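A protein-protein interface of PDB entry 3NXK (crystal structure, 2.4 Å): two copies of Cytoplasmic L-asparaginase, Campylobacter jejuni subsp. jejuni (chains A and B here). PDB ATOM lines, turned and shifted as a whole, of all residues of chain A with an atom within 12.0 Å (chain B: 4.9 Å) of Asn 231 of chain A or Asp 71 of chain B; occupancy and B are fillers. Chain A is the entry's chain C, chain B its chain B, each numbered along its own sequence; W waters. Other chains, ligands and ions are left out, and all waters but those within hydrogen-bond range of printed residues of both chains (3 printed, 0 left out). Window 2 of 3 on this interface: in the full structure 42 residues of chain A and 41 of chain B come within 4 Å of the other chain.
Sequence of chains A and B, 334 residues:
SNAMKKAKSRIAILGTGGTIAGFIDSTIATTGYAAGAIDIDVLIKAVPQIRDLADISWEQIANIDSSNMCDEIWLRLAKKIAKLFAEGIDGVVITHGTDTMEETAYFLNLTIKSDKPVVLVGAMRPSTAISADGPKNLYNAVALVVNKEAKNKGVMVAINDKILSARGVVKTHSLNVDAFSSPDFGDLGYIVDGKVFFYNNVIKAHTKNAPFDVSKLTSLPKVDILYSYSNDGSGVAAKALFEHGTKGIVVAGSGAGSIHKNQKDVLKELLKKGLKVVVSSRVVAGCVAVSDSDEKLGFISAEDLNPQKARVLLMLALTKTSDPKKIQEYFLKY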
ATOM      1  N   TYR A 227       6.360 -26.447 -18.660  1.00  0.00           N
ATOM      2  CA  TYR A 227       5.861 -26.342 -20.017  1.00  0.00           C
ATOM      3  C   TYR A 227       4.755 -25.290 -19.994  1.00  0.00           C
ATOM      4  O   TYR A 227       4.121 -25.086 -18.962  1.00  0.00           O
ATOM      5  CB  TYR A 227       5.288 -27.709 -20.409  1.00  0.00           C
ATOM      6  CG  TYR A 227       5.274 -28.027 -21.892  1.00  0.00           C
ATOM      7  CD1 TYR A 227       6.405 -28.512 -22.533  1.00  0.00           C
ATOM      8  CD2 TYR A 227       4.115 -27.879 -22.640  1.00  0.00           C
ATOM      9  CE1 TYR A 227       6.384 -28.816 -23.879  1.00  0.00           C
ATOM     10  CE2 TYR A 227       4.091 -28.183 -23.995  1.00  0.00           C
ATOM     11  CZ  TYR A 227       5.222 -28.646 -24.609  1.00  0.00           C
ATOM     12  OH  TYR A 227       5.180 -28.938 -25.961  1.00  0.00           O
ATOM     13  N   SER A 228       4.514 -24.606 -21.106  1.00  0.00           N
ATOM     14  CA  SER A 228       3.382 -23.673 -21.149  1.00  0.00           C
ATOM     15  C   SER A 228       2.384 -24.045 -22.232  1.00  0.00           C
ATOM     16  O   SER A 228       2.762 -24.486 -23.305  1.00  0.00           O
ATOM     17  CB  SER A 228       3.834 -22.227 -21.329  1.00  0.00           C
ATOM     18  OG  SER A 228       2.703 -21.359 -21.359  1.00  0.00           O
ATOM     19  N   TYR A 229       1.102 -23.859 -21.939  1.00  0.00           N
ATOM     20  CA  TYR A 229       0.032 -24.290 -22.829  1.00  0.00           C
ATOM     21  C   TYR A 229      -1.279 -23.574 -22.455  1.00  0.00           C
ATOM     22  O   TYR A 229      -1.344 -22.847 -21.463  1.00  0.00           O
ATOM     23  CB  TYR A 229      -0.128 -25.812 -22.731  1.00  0.00           C
ATOM     24  CG  TYR A 229      -0.159 -26.278 -21.297  1.00  0.00           C
ATOM     25  CD1 TYR A 229      -1.371 -26.438 -20.629  1.00  0.00           C
ATOM     26  CD2 TYR A 229       1.023 -26.512 -20.588  1.00  0.00           C
ATOM     27  CE1 TYR A 229      -1.410 -26.827 -19.302  1.00  0.00           C
ATOM     28  CE2 TYR A 229       0.993 -26.893 -19.253  1.00  0.00           C
ATOM     29  CZ  TYR A 229      -0.228 -27.046 -18.619  1.00  0.00           C
ATOM     30  OH  TYR A 229      -0.279 -27.442 -17.307  1.00  0.00           O
ATOM     31  N   SER A 230      -2.316 -23.773 -23.258  1.00  0.00           N
ATOM     32  CA  SER A 230      -3.596 -23.126 -23.035  1.00  0.00           C
ATOM     33  C   SER A 230      -4.165 -23.520 -21.684  1.00  0.00           C
ATOM     34  O   SER A 230      -4.086 -24.683 -21.295  1.00  0.00           O
ATOM     35  CB  SER A 230      -4.571 -23.513 -24.154  1.00  0.00           C
ATOM     36  OG  SER A 230      -5.874 -23.032 -23.893  1.00  0.00           O
ATOM     37  N   ASN A 231      -4.751 -22.558 -20.973  1.00  0.00           N
ATOM     38  CA  ASN A 231      -5.357 -22.834 -19.674  1.00  0.00           C
ATOM     39  C   ASN A 231      -4.317 -23.403 -18.705  1.00  0.00           C
ATOM     40  O   ASN A 231      -4.618 -24.238 -17.843  1.00  0.00           O
ATOM     41  CB  ASN A 231      -6.519 -23.824 -19.838  1.00  0.00           C
ATOM     42  CG  ASN A 231      -7.670 -23.539 -18.881  1.00  0.00           C
ATOM     43  OD1 ASN A 231      -8.664 -22.909 -19.251  1.00  0.00           O
ATOM     44  ND2 ASN A 231      -7.540 -23.997 -17.656  1.00  0.00           N
ATOM     45  N   ASP A 232      -3.087 -22.937 -18.865  1.00  0.00           N
ATOM     46  CA  ASP A 232      -1.917 -23.498 -18.195  1.00  0.00           C
ATOM     47  C   ASP A 232      -2.141 -23.599 -16.677  1.00  0.00           C
ATOM     48  O   ASP A 232      -2.574 -22.645 -16.039  1.00  0.00           O
ATOM     49  CB  ASP A 232      -0.709 -22.618 -18.565  1.00  0.00           C
ATOM     50  CG  ASP A 232       0.592 -23.038 -17.894  1.00  0.00           C
ATOM     51  OD1 ASP A 232       0.574 -23.880 -16.969  1.00  0.00           O
ATOM     52  OD2 ASP A 232       1.645 -22.478 -18.288  1.00  0.00           O
ATOM     53  N   GLY A 233      -1.864 -24.765 -16.103  1.00  0.00           N
ATOM     54  CA  GLY A 233      -1.990 -24.934 -14.662  1.00  0.00           C
ATOM     55  C   GLY A 233      -0.661 -25.055 -13.925  1.00  0.00           C
ATOM     56  O   GLY A 233      -0.629 -25.404 -12.744  1.00  0.00           O
ATOM     57  N   SER A 234       0.435 -24.742 -14.611  1.00  0.00           N
ATOM     58  CA  SER A 234       1.787 -24.959 -14.076  1.00  0.00           C
ATOM     59  C   SER A 234       2.183 -24.109 -12.874  1.00  0.00           C
ATOM     60  O   SER A 234       3.146 -24.438 -12.178  1.00  0.00           O
ATOM     61  CB  SER A 234       2.831 -24.756 -15.174  1.00  0.00           C
ATOM     62  OG  SER A 234       2.575 -25.608 -16.272  1.00  0.00           O
ATOM     63  N   GLY A 235       1.473 -23.009 -12.644  1.00  0.00           N
ATOM     64  CA  GLY A 235       1.736 -22.171 -11.485  1.00  0.00           C
ATOM     65  C   GLY A 235       1.859 -23.006 -10.221  1.00  0.00           C
ATOM     66  O   GLY A 235       2.775 -22.818  -9.419  1.00  0.00           O
ATOM     67  N   VAL A 236       0.937 -23.945 -10.049  1.00  0.00           N
ATOM     68  CA  VAL A 236       0.959 -24.831  -8.896  1.00  0.00           C
ATOM     69  C   VAL A 236       2.239 -25.663  -8.857  1.00  0.00           C
ATOM     70  O   VAL A 236       2.769 -25.965  -7.783  1.00  0.00           O
ATOM     71  CB  VAL A 236      -0.245 -25.779  -8.908  1.00  0.00           C
ATOM     72  CG1 VAL A 236      -0.007 -26.946  -7.966  1.00  0.00           C
ATOM     73  CG2 VAL A 236      -1.506 -25.029  -8.535  1.00  0.00           C
ATOM     74  N   ALA A 237       2.744 -26.035 -10.029  1.00  0.00           N
ATOM     75  CA  ALA A 237       3.976 -26.813 -10.082  1.00  0.00           C
ATOM     76  C   ALA A 237       5.200 -25.972  -9.732  1.00  0.00           C
ATOM     77  O   ALA A 237       6.136 -26.444  -9.069  1.00  0.00           O
ATOM     78  CB  ALA A 237       4.132 -27.440 -11.438  1.00  0.00           C
ATOM     79  N   ALA A 252       9.343 -24.000 -20.982  1.00  0.00           N
ATOM     80  CA  ALA A 252       9.152 -24.179 -22.417  1.00  0.00           C
ATOM     81  C   ALA A 252       7.939 -23.378 -22.853  1.00  0.00           C
ATOM     82  O   ALA A 252       6.819 -23.871 -22.827  1.00  0.00           O
ATOM     83  CB  ALA A 252       8.955 -25.656 -22.752  1.00  0.00           C
ATOM     84  N   GLY A 253       8.144 -22.131 -23.232  1.00  0.00           N
ATOM     85  CA  GLY A 253       7.006 -21.316 -23.603  1.00  0.00           C
ATOM     86  C   GLY A 253       6.475 -21.670 -24.979  1.00  0.00           C
ATOM     87  O   GLY A 253       7.113 -22.393 -25.745  1.00  0.00           O
ATOM     88  N   SER A 254       5.293 -21.154 -25.286  1.00  0.00           N
ATOM     89  CA  SER A 254       4.719 -21.275 -26.610  1.00  0.00           C
ATOM     90  C   SER A 254       5.342 -20.210 -27.495  1.00  0.00           C
ATOM     91  O   SER A 254       5.752 -19.153 -27.016  1.00  0.00           O
ATOM     92  CB  SER A 254       3.219 -21.065 -26.529  1.00  0.00           C
ATOM     93  OG  SER A 254       2.952 -20.099 -25.544  1.00  0.00           O
ATOM     94  N   SER A 258       6.590 -17.231 -24.879  1.00  0.00           N
ATOM     95  CA  SER A 258       5.401 -16.724 -24.224  1.00  0.00           C
ATOM     96  C   SER A 258       5.033 -17.671 -23.099  1.00  0.00           C
ATOM     97  O   SER A 258       5.047 -18.887 -23.273  1.00  0.00           O
ATOM     98  CB  SER A 258       4.239 -16.611 -25.214  1.00  0.00           C
ATOM     99  OG  SER A 258       4.527 -15.699 -26.259  1.00  0.00           O
ATOM    100  N   ILE A 259       4.728 -17.114 -21.935  1.00  0.00           N
ATOM    101  CA  ILE A 259       4.353 -17.924 -20.797  1.00  0.00           C
ATOM    102  C   ILE A 259       2.944 -17.525 -20.405  1.00  0.00           C
ATOM    103  O   ILE A 259       2.661 -16.344 -20.244  1.00  0.00           O
ATOM    104  CB  ILE A 259       5.337 -17.755 -19.616  1.00  0.00           C
ATOM    105  CG1 ILE A 259       6.765 -18.049 -20.084  1.00  0.00           C
ATOM    106  CG2 ILE A 259       4.966 -18.692 -18.478  1.00  0.00           C
ATOM    107  CD1 ILE A 259       7.838 -17.879 -19.008  1.00  0.00           C
ATOM    108  N   HIS A 260       2.049 -18.503 -20.300  1.00  0.00           N
ATOM    109  CA  HIS A 260       0.679 -18.222 -19.895  1.00  0.00           C
ATOM    110  C   HIS A 260       0.649 -17.403 -18.617  1.00  0.00           C
ATOM    111  O   HIS A 260       1.326 -17.732 -17.635  1.00  0.00           O
ATOM    112  CB  HIS A 260      -0.115 -19.513 -19.663  1.00  0.00           C
ATOM    113  CG  HIS A 260      -1.598 -19.306 -19.650  1.00  0.00           C
ATOM    114  ND1 HIS A 260      -2.265 -18.759 -18.574  1.00  0.00           N
ATOM    115  CD2 HIS A 260      -2.538 -19.537 -20.599  1.00  0.00           C
ATOM    116  CE1 HIS A 260      -3.552 -18.662 -18.862  1.00  0.00           C
ATOM    117  NE2 HIS A 260      -3.747 -19.137 -20.082  1.00  0.00           N
ATOM    118  N   LYS A 261      -0.160 -16.349 -18.639  1.00  0.00           N
ATOM    119  CA  LYS A 261      -0.414 -15.474 -17.489  1.00  0.00           C
ATOM    120  C   LYS A 261      -0.648 -16.205 -16.151  1.00  0.00           C
ATOM    121  O   LYS A 261      -0.322 -15.682 -15.092  1.00  0.00           O
ATOM    122  CB  LYS A 261      -1.610 -14.575 -17.821  1.00  0.00           C
ATOM    123  CG  LYS A 261      -1.848 -13.386 -16.903  1.00  0.00           C
ATOM    124  CD  LYS A 261      -3.073 -12.608 -17.393  1.00  0.00           C
ATOM    125  CE  LYS A 261      -4.155 -13.565 -17.936  1.00  0.00           C
ATOM    126  NZ  LYS A 261      -5.338 -12.883 -18.553  1.00  0.00           N
ATOM    127  N   ASN A 262      -1.221 -17.404 -16.181  1.00  0.00           N
ATOM    128  CA  ASN A 262      -1.405 -18.152 -14.935  1.00  0.00           C
ATOM    129  C   ASN A 262      -0.073 -18.598 -14.311  1.00  0.00           C
ATOM    130  O   ASN A 262       0.131 -18.468 -13.100  1.00  0.00           O
ATOM    131  CB  ASN A 262      -2.319 -19.364 -15.130  1.00  0.00           C
ATOM    132  CG  ASN A 262      -3.741 -18.977 -15.532  1.00  0.00           C
ATOM    133  OD1 ASN A 262      -4.216 -17.875 -15.233  1.00  0.00           O
ATOM    134  ND2 ASN A 262      -4.432 -19.898 -16.206  1.00  0.00           N
ATOM    135  N   GLN A 263       0.823 -19.137 -15.140  1.00  0.00           N
ATOM    136  CA  GLN A 263       2.140 -19.554 -14.670  1.00  0.00           C
ATOM    137  C   GLN A 263       3.052 -18.353 -14.407  1.00  0.00           C
ATOM    138  O   GLN A 263       3.724 -18.284 -13.376  1.00  0.00           O
ATOM    139  CB  GLN A 263       2.809 -20.517 -15.670  1.00  0.00           C
ATOM    140  CG  GLN A 263       4.291 -20.742 -15.373  1.00  0.00           C
ATOM    141  CD  GLN A 263       4.892 -21.933 -16.090  1.00  0.00           C
ATOM    142  OE1 GLN A 263       4.258 -22.569 -16.937  1.00  0.00           O
ATOM    143  NE2 GLN A 263       6.131 -22.244 -15.747  1.00  0.00           N
ATOM    144  N   LYS A 264       3.060 -17.411 -15.346  1.00  0.00           N
ATOM    145  CA  LYS A 264       3.970 -16.275 -15.292  1.00  0.00           C
ATOM    146  C   LYS A 264       3.745 -15.416 -14.052  1.00  0.00           C
ATOM    147  O   LYS A 264       4.694 -14.893 -13.476  1.00  0.00           O
ATOM    148  CB  LYS A 264       3.840 -15.428 -16.556  1.00  0.00           C
ATOM    149  CG  LYS A 264       5.004 -14.477 -16.790  1.00  0.00           C
ATOM    150  CD  LYS A 264       4.859 -13.797 -18.143  1.00  0.00           C
ATOM    151  CE  LYS A 264       5.986 -12.818 -18.409  1.00  0.00           C
ATOM    152  NZ  LYS A 264       5.804 -12.144 -19.726  1.00  0.00           N
ATOM    153  N   ASP A 265       2.496 -15.278 -13.626  1.00  0.00           N
ATOM    154  CA  ASP A 265       2.232 -14.531 -12.404  1.00  0.00           C
ATOM    155  C   ASP A 265       2.904 -15.178 -11.187  1.00  0.00           C
ATOM    156  O   ASP A 265       3.495 -14.481 -10.359  1.00  0.00           O
ATOM    157  CB  ASP A 265       0.732 -14.352 -12.184  1.00  0.00           C
ATOM    158  CG  ASP A 265       0.147 -13.241 -13.043  1.00  0.00           C
ATOM    159  OD1 ASP A 265       0.940 -12.441 -13.593  1.00  0.00           O
ATOM    160  OD2 ASP A 265      -1.099 -13.165 -13.155  1.00  0.00           O
ATOM    161  N   VAL A 266       2.826 -16.504 -11.091  1.00  0.00           N
ATOM    162  CA  VAL A 266       3.531 -17.244 -10.044  1.00  0.00           C
ATOM    163  C   VAL A 266       5.047 -17.094 -10.197  1.00  0.00           C
ATOM    164  O   VAL A 266       5.764 -16.772  -9.244  1.00  0.00           O
ATOM    165  CB  VAL A 266       3.158 -18.747 -10.073  1.00  0.00           C
ATOM    166  CG1 VAL A 266       4.103 -19.569  -9.188  1.00  0.00           C
ATOM    167  CG2 VAL A 266       1.687 -18.952  -9.661  1.00  0.00           C
ATOM    168  N   ARG A 282       8.961 -24.430 -26.686  1.00  0.00           N
ATOM    169  CA  ARG A 282       8.475 -25.774 -26.964  1.00  0.00           C
ATOM    170  C   ARG A 282       8.476 -25.974 -28.468  1.00  0.00           C
ATOM    171  O   ARG A 282       8.254 -27.081 -28.954  1.00  0.00           O
ATOM    172  CB  ARG A 282       7.047 -25.913 -26.446  1.00  0.00           C
ATOM    173  CG  ARG A 282       6.052 -25.031 -27.196  1.00  0.00           C
ATOM    174  CD  ARG A 282       4.694 -25.097 -26.565  1.00  0.00           C
ATOM    175  NE  ARG A 282       3.640 -24.720 -27.492  1.00  0.00           N
ATOM    176  CZ  ARG A 282       2.344 -24.779 -27.203  1.00  0.00           C
ATOM    177  NH1 ARG A 282       1.941 -25.212 -26.007  1.00  0.00           N
ATOM    178  NH2 ARG A 282       1.451 -24.430 -28.113  1.00  0.00           N
ATOM    179  N   MET B  69      -4.603 -18.242 -24.038  1.00  0.00           N
ATOM    180  CA  MET B  69      -5.792 -19.019 -24.364  1.00  0.00           C
ATOM    181  C   MET B  69      -6.267 -19.813 -23.140  1.00  0.00           C
ATOM    182  O   MET B  69      -5.480 -20.158 -22.258  1.00  0.00           O
ATOM    183  CB  MET B  69      -5.482 -19.952 -25.528  1.00  0.00           C
ATOM    184  CG  MET B  69      -6.688 -20.628 -26.134  1.00  0.00           C
ATOM    185  SD  MET B  69      -8.036 -19.362 -26.765  1.00  0.00           S
ATOM    186  CE  MET B  69      -6.809 -18.064 -27.598  1.00  0.00           C
ATOM    187  N   CYS B  70      -7.564 -20.090 -23.089  1.00  0.00           N
ATOM    188  CA  CYS B  70      -8.157 -20.831 -21.983  1.00  0.00           C
ATOM    189  C   CYS B  70      -9.381 -21.640 -22.452  1.00  0.00           C
ATOM    190  O   CYS B  70      -9.831 -21.480 -23.592  1.00  0.00           O
ATOM    191  CB  CYS B  70      -8.529 -19.875 -20.839  1.00  0.00           C
ATOM    192  SG  CYS B  70      -9.777 -18.630 -21.270  1.00  0.00           S
ATOM    193  N   ASP B  71      -9.898 -22.502 -21.565  1.00  0.00           N
ATOM    194  CA  ASP B  71     -11.029 -23.402 -21.843  1.00  0.00           C
ATOM    195  C   ASP B  71     -12.320 -22.680 -22.199  1.00  0.00           C
ATOM    196  O   ASP B  71     -13.101 -23.144 -23.031  1.00  0.00           O
ATOM    197  CB  ASP B  71     -11.336 -24.275 -20.626  1.00  0.00           C
ATOM    198  CG  ASP B  71     -10.223 -25.260 -20.303  1.00  0.00           C
ATOM    199  OD1 ASP B  71      -9.312 -25.487 -21.137  1.00  0.00           O
ATOM    200  OD2 ASP B  71     -10.268 -25.825 -19.192  1.00  0.00           O
ATOM    201  N   GLU B  72     -12.559 -21.563 -21.532  1.00  0.00           N
ATOM    202  CA  GLU B  72     -13.813 -20.850 -21.691  1.00  0.00           C
ATOM    203  C   GLU B  72     -13.946 -20.315 -23.124  1.00  0.00           C
ATOM    204  O   GLU B  72     -15.013 -20.404 -23.739  1.00  0.00           O
ATOM    205  CB  GLU B  72     -13.926 -19.733 -20.651  1.00  0.00           C
ATOM    206  CG  GLU B  72     -15.310 -19.108 -20.547  1.00  0.00           C
ATOM    207  CD  GLU B  72     -15.443 -17.817 -21.351  1.00  0.00           C
ATOM    208  OE1 GLU B  72     -14.419 -17.343 -21.897  1.00  0.00           O
ATOM    209  OE2 GLU B  72     -16.571 -17.271 -21.432  1.00  0.00           O
ATOM    210  N   ILE B  73     -12.854 -19.789 -23.663  1.00  0.00           N
ATOM    211  CA  ILE B  73     -12.897 -19.268 -25.016  1.00  0.00           C
ATOM    212  C   ILE B  73     -13.151 -20.404 -25.999  1.00  0.00           C
ATOM    213  O   ILE B  73     -13.976 -20.266 -26.907  1.00  0.00           O
ATOM    214  CB  ILE B  73     -11.632 -18.457 -25.358  1.00  0.00           C
ATOM    215  CG1 ILE B  73     -11.568 -17.197 -24.481  1.00  0.00           C
ATOM    216  CG2 ILE B  73     -11.607 -18.075 -26.830  1.00  0.00           C
ATOM    217  CD1 ILE B  73     -10.225 -16.506 -24.525  1.00  0.00           C
ATOM    218  N   TRP B  74     -12.475 -21.534 -25.790  1.00  0.00           N
ATOM    219  CA  TRP B  74     -12.730 -22.757 -26.562  1.00  0.00           C
ATOM    220  C   TRP B  74     -14.206 -23.169 -26.578  1.00  0.00           C
ATOM    221  O   TRP B  74     -14.768 -23.444 -27.648  1.00  0.00           O
ATOM    222  CB  TRP B  74     -11.893 -23.922 -26.038  1.00  0.00           C
ATOM    223  CG  TRP B  74     -10.435 -23.845 -26.426  1.00  0.00           C
ATOM    224  CD1 TRP B  74      -9.814 -22.842 -27.114  1.00  0.00           C
ATOM    225  CD2 TRP B  74      -9.434 -24.829 -26.163  1.00  0.00           C
ATOM    226  NE1 TRP B  74      -8.477 -23.139 -27.279  1.00  0.00           N
ATOM    227  CE2 TRP B  74      -8.224 -24.353 -26.698  1.00  0.00           C
ATOM    228  CE3 TRP B  74      -9.444 -26.066 -25.512  1.00  0.00           C
ATOM    229  CZ2 TRP B  74      -7.035 -25.074 -26.604  1.00  0.00           C
ATOM    230  CZ3 TRP B  74      -8.276 -26.774 -25.425  1.00  0.00           C
ATOM    231  CH2 TRP B  74      -7.085 -26.280 -25.968  1.00  0.00           C
ATOM    232  N   LEU B  75     -14.835 -23.206 -25.403  1.00  0.00           N
ATOM    233  CA  LEU B  75     -16.235 -23.621 -25.315  1.00  0.00           C
ATOM    234  C   LEU B  75     -17.127 -22.623 -26.044  1.00  0.00           C
ATOM    235  O   LEU B  75     -18.029 -23.005 -26.804  1.00  0.00           O
ATOM    236  CB  LEU B  75     -16.680 -23.824 -23.858  1.00  0.00           C
ATOM    237  CG  LEU B  75     -16.129 -25.092 -23.177  1.00  0.00           C
ATOM    238  CD1 LEU B  75     -16.354 -25.093 -21.671  1.00  0.00           C
ATOM    239  CD2 LEU B  75     -16.713 -26.342 -23.790  1.00  0.00           C
ATOM    240  N   LEU B 220     -14.159 -27.834 -18.464  1.00  0.00           N
ATOM    241  CA  LEU B 220     -13.479 -29.020 -18.970  1.00  0.00           C
ATOM    242  C   LEU B 220     -12.639 -29.665 -17.881  1.00  0.00           C
ATOM    243  O   LEU B 220     -12.239 -28.998 -16.926  1.00  0.00           O
ATOM    244  CB  LEU B 220     -12.614 -28.675 -20.192  1.00  0.00           C
ATOM    245  CG  LEU B 220     -13.413 -28.230 -21.418  1.00  0.00           C
ATOM    246  CD1 LEU B 220     -12.501 -27.769 -22.534  1.00  0.00           C
ATOM    247  CD2 LEU B 220     -14.305 -29.360 -21.878  1.00  0.00           C
ATOM    248  N   ASP B 224      -2.994 -31.374 -17.146  1.00  0.00           N
ATOM    249  CA  ASP B 224      -1.778 -30.584 -17.140  1.00  0.00           C
ATOM    250  C   ASP B 224      -0.620 -31.290 -17.847  1.00  0.00           C
ATOM    251  O   ASP B 224      -0.758 -32.441 -18.282  1.00  0.00           O
ATOM    252  CB  ASP B 224      -1.473 -30.140 -15.716  1.00  0.00           C
ATOM    253  CG  ASP B 224      -2.469 -29.077 -15.234  1.00  0.00           C
ATOM    254  OD1 ASP B 224      -2.288 -27.905 -15.636  1.00  0.00           O
ATOM    255  OD2 ASP B 224      -3.447 -29.388 -14.509  1.00  0.00           O
ATOM    256  N   ARG B 311      -3.067 -33.135 -24.739  1.00  0.00           N
ATOM    257  CA  ARG B 311      -3.876 -32.587 -23.683  1.00  0.00           C
ATOM    258  C   ARG B 311      -5.314 -32.385 -24.187  1.00  0.00           C
ATOM    259  O   ARG B 311      -6.274 -32.740 -23.489  1.00  0.00           O
ATOM    260  CB  ARG B 311      -3.304 -31.261 -23.182  1.00  0.00           C
ATOM    261  CG  ARG B 311      -4.304 -30.491 -22.354  1.00  0.00           C
ATOM    262  CD  ARG B 311      -3.748 -29.198 -21.836  1.00  0.00           C
ATOM    263  NE  ARG B 311      -4.694 -28.583 -20.911  1.00  0.00           N
ATOM    264  CZ  ARG B 311      -5.566 -27.639 -21.244  1.00  0.00           C
ATOM    265  NH1 ARG B 311      -5.596 -27.150 -22.479  1.00  0.00           N
ATOM    266  NH2 ARG B 311      -6.398 -27.168 -20.327  1.00  0.00           N
ATOM    267  N   MET B 315      -8.418 -34.503 -22.427  1.00  0.00           N
ATOM    268  CA  MET B 315      -9.408 -33.670 -21.782  1.00  0.00           C
ATOM    269  C   MET B 315     -10.826 -33.937 -22.314  1.00  0.00           C
ATOM    270  O   MET B 315     -11.796 -33.963 -21.546  1.00  0.00           O
ATOM    271  CB  MET B 315      -9.007 -32.216 -22.020  1.00  0.00           C
ATOM    272  CG  MET B 315      -9.865 -31.168 -21.382  1.00  0.00           C
ATOM    273  SD  MET B 315      -8.829 -29.493 -21.366  1.00  0.00           S
ATOM    274  CE  MET B 315      -8.299 -29.486 -23.221  1.00  0.00           C
HETATM  275  O   HOH W   1     -11.252 -21.426 -19.102  1.00  0.00           O
HETATM  276  O   HOH W   2      -7.618 -24.943 -22.886  1.00  0.00           O
HETATM  277  O   HOH W   3      -4.962 -26.764 -16.613  1.00  0.00           O
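The backbone carbonyl oxygen (O) of Met 69 of chain B lies close to the side-chain hydroxyl (OG) of Ser 230 of chain A (3.3 Å).
N of Asn 231 of chain A is in hydrogen-bond range of O of Met 69 of chain B, at 2.8 Å.
The backbone carbonyl oxygen (O) of Met 69 of chain B sits at hydrogen-bond distance from a ring nitrogen (NE2) of His 260 of chain A.
N of Cys 70 of chain B lies within hydrogen-bond range of OG of Ser 230 of chain A, 3.5 Å away.
The backbone NH (N) of Asp 71 of chain B lies within hydrogen-bond range of the side-chain amide oxygen (OD1) of Asn 231 of chain A (2.7 Å).
OD1 of Asp 224 of chain B is in hydrogen-bond range of OH of Tyr 229 of chain A (2.7 Å).
The side-chain carboxylate (OD1) of Asp 224 of chain B lies close to the backbone NH (N) of Gly 233 of chain A (3.2 Å).
The guanidinium group (NH1) of Arg 311 of chain B lies within hydrogen-bond range of the backbone carbonyl oxygen (O) of Ser 230 of chain A (3.1 Å).
The guanidinium group of Arg 311 of chain B is in salt-bridge range of the side-chain carboxylate of Asp 71 of chain B (3.5 Å).
NH2 of Arg 311 of chain B is in hydrogen-bond range of SD of Met 315 of chain B (3.5 Å).
N of His 260 of chain A lies within hydrogen-bond range of OG of Ser 228 of chain A, at 3.1 Å.
N of Gly 233 of chain A is in hydrogen-bond range of OH of Tyr 229 of chain A.
The backbone NH (N) of Asn 262 of chain A lies within hydrogen-bond range of a ring nitrogen (ND1) of His 260 of chain A (2.9 Å).
Among the printed residues, pairs that only touch across the chains: Asn 231 of chain A with Arg 311 of chain B (3.4 Å), Asn 231 of chain A with Cys 70 of chain B (3.4 Å), Ser 230 of chain A with Trp 74 of chain B (3.6 Å) and Tyr 229 of chain A with Arg 311 of chain B (3.8 Å).
Of chain B, only Met 69, Cys 70, Asp 71 and Arg 311 come within 4 Å of Asn 231 of chain A.
Asp 71 of chain B touches one residue of chain A.
No residue of chain A comes within 4 Å of Glu 72 of chain B.
Trp 74 of chain B touches just one residue of chain A: Ser 230 (3.6 Å).
No residue of chain A comes within 4 Å of Leu 220 of chain B.
Of the printed residues of chain A, Met 69 of chain B touches Ser 230, Asn 231 and His 260.
Of the printed residues of chain B, Ser 230 of chain A touches Met 69 (3.3 Å), Cys 70 (3.5 Å), Trp 74 (3.6 Å) and Arg 311 (3.1 Å).
Of the printed residues of chain A, Asp 224 of chain B touches Tyr 229 and Gly 233.
Printed residues of chain B within 4 Å of His 260 of chain A: Met 69 (3.0 Å).
Printed residues of chain B within 4 Å of Tyr 229 of chain A: Asp 224 (2.7 Å) and Arg 311 (3.8 Å).
Ser 258 of chain A touches none of the printed residues of chain B.
The nearest residue of chain B that does not touch Asn 231 of chain A is Glu 72 of chain B (4.7 Å).
The nearest residue of chain A that does not touch Asp 71 of chain B is Ser 230 of chain A (4.7 Å).
Of the 11 printed residues of chain B, 6 touch a printed residue of chain A.
Hydrophobic or aromatic side chains of chain B that line the printed part of chain A: Met 69 and Trp 74.
Of the 24 printed residues of chain A, 5 touch a printed residue of chain B.
Hydrophobic or aromatic side chains of chain A within 4 Å of the printed part of chain B: Tyr 229 and His 260.
Among the printed residues, 12 pairs touch across the chains.
Among the printed residues, no Asp or Glu carboxylate lies within 4 Å of a Lys or Arg side-chain nitrogen of the other chain.
No position is printed for both chains.
Of the 12 pairs that touch across the chains among the printed residues, none has its exchanged pair printed and touching as well.
Water W2 lies within hydrogen-bond range of OD1 of Asp 71 of chain B, OG of Ser 230 of chain A and NH1 of Arg 311 of chain B.
Water W1 lies within hydrogen-bond range of the backbone NH (N) of Glu 72 of chain B, the side-chain amide oxygen (OD1) of Asn 231 of chain A and the backbone NH (N) of Asp 71 of chain B.
Water W3 bridges O of Asn 231 of chain A and OD1 of Asp 224 of chain B.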
